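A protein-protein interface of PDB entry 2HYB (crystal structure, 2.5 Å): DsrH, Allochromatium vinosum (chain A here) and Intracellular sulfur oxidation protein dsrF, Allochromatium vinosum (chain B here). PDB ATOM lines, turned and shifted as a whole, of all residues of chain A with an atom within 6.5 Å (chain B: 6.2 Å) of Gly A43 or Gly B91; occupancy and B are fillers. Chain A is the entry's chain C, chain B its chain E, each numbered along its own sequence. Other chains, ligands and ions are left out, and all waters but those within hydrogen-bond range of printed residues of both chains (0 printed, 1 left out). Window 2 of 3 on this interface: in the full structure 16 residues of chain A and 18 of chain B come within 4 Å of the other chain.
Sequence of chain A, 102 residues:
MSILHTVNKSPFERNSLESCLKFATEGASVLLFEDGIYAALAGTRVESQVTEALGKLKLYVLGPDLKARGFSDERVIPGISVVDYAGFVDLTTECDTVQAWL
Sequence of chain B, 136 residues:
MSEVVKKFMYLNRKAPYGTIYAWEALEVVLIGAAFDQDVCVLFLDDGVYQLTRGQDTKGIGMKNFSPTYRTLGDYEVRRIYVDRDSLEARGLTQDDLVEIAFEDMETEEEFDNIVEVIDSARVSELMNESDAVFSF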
ATOM      1  N   LEU A  41      -6.645   3.080  -5.285  1.00  0.00           N
ATOM      2  CA  LEU A  41      -7.612   2.031  -5.589  1.00  0.00           C
ATOM      3  C   LEU A  41      -7.827   1.816  -7.081  1.00  0.00           C
ATOM      4  O   LEU A  41      -8.035   2.762  -7.834  1.00  0.00           O
ATOM      5  CB  LEU A  41      -8.958   2.350  -4.926  1.00  0.00           C
ATOM      6  CG  LEU A  41      -8.924   2.398  -3.396  1.00  0.00           C
ATOM      7  CD1 LEU A  41     -10.309   2.733  -2.848  1.00  0.00           C
ATOM      8  CD2 LEU A  41      -8.426   1.044  -2.864  1.00  0.00           C
ATOM      9  N   ALA A  42      -7.772   0.563  -7.508  1.00  0.00           N
ATOM     10  CA  ALA A  42      -7.991   0.239  -8.910  1.00  0.00           C
ATOM     11  C   ALA A  42      -9.442   0.554  -9.280  1.00  0.00           C
ATOM     12  O   ALA A  42     -10.330   0.465  -8.434  1.00  0.00           O
ATOM     13  CB  ALA A  42      -7.713  -1.242  -9.144  1.00  0.00           C
ATOM     14  N   GLY A  43      -9.687   0.940 -10.529  1.00  0.00           N
ATOM     15  CA  GLY A  43     -11.055   1.200 -10.943  1.00  0.00           C
ATOM     16  C   GLY A  43     -11.605   2.615 -10.923  1.00  0.00           C
ATOM     17  O   GLY A  43     -12.547   2.907 -11.665  1.00  0.00           O
ATOM     18  N   THR A  44     -11.038   3.502 -10.107  1.00  0.00           N
ATOM     19  CA  THR A  44     -11.544   4.870 -10.045  1.00  0.00           C
ATOM     20  C   THR A  44     -11.211   5.711 -11.265  1.00  0.00           C
ATOM     21  O   THR A  44     -10.362   5.362 -12.083  1.00  0.00           O
ATOM     22  CB  THR A  44     -11.009   5.655  -8.826  1.00  0.00           C
ATOM     23  OG1 THR A  44      -9.735   6.219  -9.150  1.00  0.00           O
ATOM     24  CG2 THR A  44     -10.872   4.750  -7.608  1.00  0.00           C
ATOM     25  N   ARG A  45     -11.895   6.842 -11.341  1.00  0.00           N
ATOM     26  CA  ARG A  45     -11.752   7.831 -12.391  1.00  0.00           C
ATOM     27  C   ARG A  45     -10.287   8.215 -12.627  1.00  0.00           C
ATOM     28  O   ARG A  45      -9.901   8.542 -13.747  1.00  0.00           O
ATOM     29  CB  ARG A  45     -12.529   9.069 -11.964  1.00  0.00           C
ATOM     30  CG  ARG A  45     -13.060   9.921 -13.077  1.00  0.00           C
ATOM     31  CD  ARG A  45     -13.774  11.101 -12.488  1.00  0.00           C
ATOM     32  NE  ARG A  45     -12.857  11.866 -11.661  1.00  0.00           N
ATOM     33  CZ  ARG A  45     -13.233  12.573 -10.611  1.00  0.00           C
ATOM     34  NH1 ARG A  45     -14.512  12.606 -10.262  1.00  0.00           N
ATOM     35  NH2 ARG A  45     -12.332  13.247  -9.914  1.00  0.00           N
ATOM     36  N   VAL A  46      -9.475   8.159 -11.573  1.00  0.00           N
ATOM     37  CA  VAL A  46      -8.073   8.549 -11.669  1.00  0.00           C
ATOM     38  C   VAL A  46      -7.035   7.431 -11.714  1.00  0.00           C
ATOM     39  O   VAL A  46      -5.846   7.664 -11.499  1.00  0.00           O
ATOM     40  CB  VAL A  46      -7.710   9.521 -10.518  1.00  0.00           C
ATOM     41  CG1 VAL A  46      -8.718  10.661 -10.479  1.00  0.00           C
ATOM     42  CG2 VAL A  46      -7.680   8.791  -9.180  1.00  0.00           C
ATOM     43  N   GLU A  47      -7.472   6.215 -11.992  1.00  0.00           N
ATOM     44  CA  GLU A  47      -6.533   5.114 -12.076  1.00  0.00           C
ATOM     45  C   GLU A  47      -5.497   5.392 -13.164  1.00  0.00           C
ATOM     46  O   GLU A  47      -4.296   5.208 -12.954  1.00  0.00           O
ATOM     47  CB  GLU A  47      -7.274   3.830 -12.407  1.00  0.00           C
ATOM     48  CG  GLU A  47      -6.376   2.627 -12.571  1.00  0.00           C
ATOM     49  CD  GLU A  47      -7.175   1.378 -12.814  1.00  0.00           C
ATOM     50  OE1 GLU A  47      -6.801   0.323 -12.243  1.00  0.00           O
ATOM     51  OE2 GLU A  47      -8.173   1.460 -13.569  1.00  0.00           O
ATOM     52  N   ARG A  75      -7.233  -4.510  -3.653  1.00  0.00           N
ATOM     53  CA  ARG A  75      -7.999  -3.482  -4.356  1.00  0.00           C
ATOM     54  C   ARG A  75      -7.085  -2.357  -4.868  1.00  0.00           C
ATOM     55  O   ARG A  75      -7.546  -1.435  -5.551  1.00  0.00           O
ATOM     56  CB  ARG A  75      -9.080  -2.897  -3.427  1.00  0.00           C
ATOM     57  CG  ARG A  75      -9.951  -3.935  -2.694  1.00  0.00           C
ATOM     58  CD  ARG A  75     -10.925  -4.635  -3.620  1.00  0.00           C
ATOM     59  NE  ARG A  75     -12.017  -3.779  -4.086  1.00  0.00           N
ATOM     60  CZ  ARG A  75     -13.059  -3.402  -3.344  1.00  0.00           C
ATOM     61  NH1 ARG A  75     -13.174  -3.793  -2.073  1.00  0.00           N
ATOM     62  NH2 ARG A  75     -14.014  -2.650  -3.884  1.00  0.00           N
ATOM     63  N   ILE A  77      -3.891  -0.512  -6.973  1.00  0.00           N
ATOM     64  CA  ILE A  77      -3.326  -0.461  -8.322  1.00  0.00           C
ATOM     65  C   ILE A  77      -1.948  -1.121  -8.311  1.00  0.00           C
ATOM     66  O   ILE A  77      -1.060  -0.689  -7.579  1.00  0.00           O
ATOM     67  CB  ILE A  77      -3.141   1.005  -8.800  1.00  0.00           C
ATOM     68  CG1 ILE A  77      -4.495   1.691  -8.967  1.00  0.00           C
ATOM     69  CG2 ILE A  77      -2.347   1.031 -10.089  1.00  0.00           C
ATOM     70  CD1 ILE A  77      -4.396   3.177  -9.339  1.00  0.00           C
ATOM     71  N   SER B  86     -21.547   8.667  -8.655  1.00  0.00           N
ATOM     72  CA  SER B  86     -20.448   8.700  -7.699  1.00  0.00           C
ATOM     73  C   SER B  86     -19.844   7.303  -7.566  1.00  0.00           C
ATOM     74  O   SER B  86     -18.632   7.132  -7.679  1.00  0.00           O
ATOM     75  CB  SER B  86     -20.936   9.195  -6.334  1.00  0.00           C
ATOM     76  OG  SER B  86     -21.489  10.493  -6.433  1.00  0.00           O
ATOM     77  N   LEU B  87     -20.686   6.303  -7.332  1.00  0.00           N
ATOM     78  CA  LEU B  87     -20.198   4.932  -7.205  1.00  0.00           C
ATOM     79  C   LEU B  87     -19.356   4.585  -8.419  1.00  0.00           C
ATOM     80  O   LEU B  87     -18.269   4.011  -8.297  1.00  0.00           O
ATOM     81  CB  LEU B  87     -21.370   3.955  -7.108  1.00  0.00           C
ATOM     82  CG  LEU B  87     -22.186   4.049  -5.818  1.00  0.00           C
ATOM     83  CD1 LEU B  87     -23.400   3.149  -5.907  1.00  0.00           C
ATOM     84  CD2 LEU B  87     -21.304   3.685  -4.628  1.00  0.00           C
ATOM     85  N   GLU B  88     -19.871   4.948  -9.590  1.00  0.00           N
ATOM     86  CA  GLU B  88     -19.202   4.692 -10.856  1.00  0.00           C
ATOM     87  C   GLU B  88     -17.818   5.350 -10.903  1.00  0.00           C
ATOM     88  O   GLU B  88     -16.804   4.663 -11.016  1.00  0.00           O
ATOM     89  CB  GLU B  88     -20.088   5.194 -12.005  1.00  0.00           C
ATOM     90  CG  GLU B  88     -19.649   4.779 -13.408  1.00  0.00           C
ATOM     91  CD  GLU B  88     -20.654   5.199 -14.479  1.00  0.00           C
ATOM     92  OE1 GLU B  88     -20.984   6.403 -14.556  1.00  0.00           O
ATOM     93  OE2 GLU B  88     -21.106   4.326 -15.251  1.00  0.00           O
ATOM     94  N   ALA B  89     -17.772   6.676 -10.812  1.00  0.00           N
ATOM     95  CA  ALA B  89     -16.491   7.376 -10.854  1.00  0.00           C
ATOM     96  C   ALA B  89     -15.507   6.763  -9.864  1.00  0.00           C
ATOM     97  O   ALA B  89     -14.301   6.743 -10.101  1.00  0.00           O
ATOM     98  CB  ALA B  89     -16.683   8.850 -10.566  1.00  0.00           C
ATOM     99  N   ARG B  90     -16.015   6.253  -8.753  1.00  0.00           N
ATOM    100  CA  ARG B  90     -15.131   5.637  -7.768  1.00  0.00           C
ATOM    101  C   ARG B  90     -14.916   4.144  -7.997  1.00  0.00           C
ATOM    102  O   ARG B  90     -14.237   3.482  -7.217  1.00  0.00           O
ATOM    103  CB  ARG B  90     -15.653   5.917  -6.359  1.00  0.00           C
ATOM    104  CG  ARG B  90     -15.545   7.383  -6.063  1.00  0.00           C
ATOM    105  CD  ARG B  90     -16.264   7.822  -4.820  1.00  0.00           C
ATOM    106  NE  ARG B  90     -16.160   9.273  -4.685  1.00  0.00           N
ATOM    107  CZ  ARG B  90     -16.762  10.148  -5.486  1.00  0.00           C
ATOM    108  NH1 ARG B  90     -17.523   9.730  -6.490  1.00  0.00           N
ATOM    109  NH2 ARG B  90     -16.596  11.447  -5.287  1.00  0.00           N
ATOM    110  N   GLY B  91     -15.486   3.637  -9.086  1.00  0.00           N
ATOM    111  CA  GLY B  91     -15.356   2.233  -9.436  1.00  0.00           C
ATOM    112  C   GLY B  91     -15.941   1.269  -8.428  1.00  0.00           C
ATOM    113  O   GLY B  91     -15.305   0.286  -8.044  1.00  0.00           O
ATOM    114  N   LEU B  92     -17.160   1.546  -7.996  1.00  0.00           N
ATOM    115  CA  LEU B  92     -17.826   0.707  -7.018  1.00  0.00           C
ATOM    116  C   LEU B  92     -19.224   0.375  -7.505  1.00  0.00           C
ATOM    117  O   LEU B  92     -19.753   1.013  -8.423  1.00  0.00           O
ATOM    118  CB  LEU B  92     -17.950   1.442  -5.686  1.00  0.00           C
ATOM    119  CG  LEU B  92     -16.712   2.078  -5.071  1.00  0.00           C
ATOM    120  CD1 LEU B  92     -17.158   2.935  -3.901  1.00  0.00           C
ATOM    121  CD2 LEU B  92     -15.722   1.021  -4.628  1.00  0.00           C
ATOM    122  N   THR B  93     -19.819  -0.627  -6.872  1.00  0.00           N
ATOM    123  CA  THR B  93     -21.168  -1.052  -7.190  1.00  0.00           C
ATOM    124  C   THR B  93     -21.847  -1.203  -5.842  1.00  0.00           C
ATOM    125  O   THR B  93     -21.186  -1.197  -4.804  1.00  0.00           O
ATOM    126  CB  THR B  93     -21.169  -2.402  -7.905  1.00  0.00           C
ATOM    127  OG1 THR B  93     -20.581  -3.396  -7.050  1.00  0.00           O
ATOM    128  CG2 THR B  93     -20.372  -2.303  -9.199  1.00  0.00           C
ATOM    129  N   ASP B  96     -20.320  -3.052  -3.029  1.00  0.00           N
ATOM    130  CA  ASP B  96     -19.241  -2.617  -2.159  1.00  0.00           C
ATOM    131  C   ASP B  96     -19.776  -2.012  -0.876  1.00  0.00           C
ATOM    132  O   ASP B  96     -19.059  -1.886   0.118  1.00  0.00           O
ATOM    133  CB  ASP B  96     -18.356  -1.625  -2.889  1.00  0.00           C
ATOM    134  CG  ASP B  96     -17.618  -2.264  -4.030  1.00  0.00           C
ATOM    135  OD1 ASP B  96     -18.038  -2.080  -5.191  1.00  0.00           O
ATOM    136  OD2 ASP B  96     -16.624  -2.971  -3.758  1.00  0.00           O
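The backbone NH (N) of Arg A45 lies within hydrogen-bond range of the backbone carbonyl oxygen (O) of Ala B89, 2.7 Å away.
The guanidinium group (NH2) of Arg A75 lies within salt-bridge range of the side-chain carboxylate (OD2) of Asp B96, at 2.6 Å.
O of Ser B86 is in hydrogen-bond range of NH1 of Arg B90, at 3.1 Å.
The backbone NH (N) of Thr B93 is in hydrogen-bond range of the side-chain carboxylate (OD1) of Asp B96 (2.8 Å).
The backbone NH (N) of Ala A42 sits at hydrogen-bond distance from the backbone carbonyl oxygen (O) of Arg A75.
N of Gly A43 sits at hydrogen-bond distance from OE1 of Glu A47 (3.4 Å).
OG1 of Thr A44 sits close to N of Val A46.
Among the printed residues, merely in contact across the chains: Gly A43 with Gly B91, Thr A44 with Ala B89 and Thr A44 with Arg B90.
Of the printed residues of chain A, Gly B91 touches Gly A43.
Printed residues of chain B within 4 Å of Thr A44: Ala B89 (3.3 Å) and Arg B90 (3.6 Å).
Of the printed residues of chain A, Arg B90 touches Thr A44 (3.6 Å).
Leu B92 touches none of the printed residues of chain A.
Leu A41 touches none of the printed residues of chain B.
The nearest residue of chain A that does not touch Gly B91 is Thr A44 (4.2 Å).
The nearest printed residue of chain A that does not touch Ala B89 is Gly A43 (4.5 Å).
Of the 9 printed residues of chain A, 4 touch a printed residue of chain B.
Printed residues of chain A that touch a printed residue of chain B: Gly A43, Thr A44, Arg A45 and Arg A75.
Of the 9 printed residues of chain B, 4 touch a printed residue of chain A.
Among the printed residues, 5 pairs touch across the chains.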
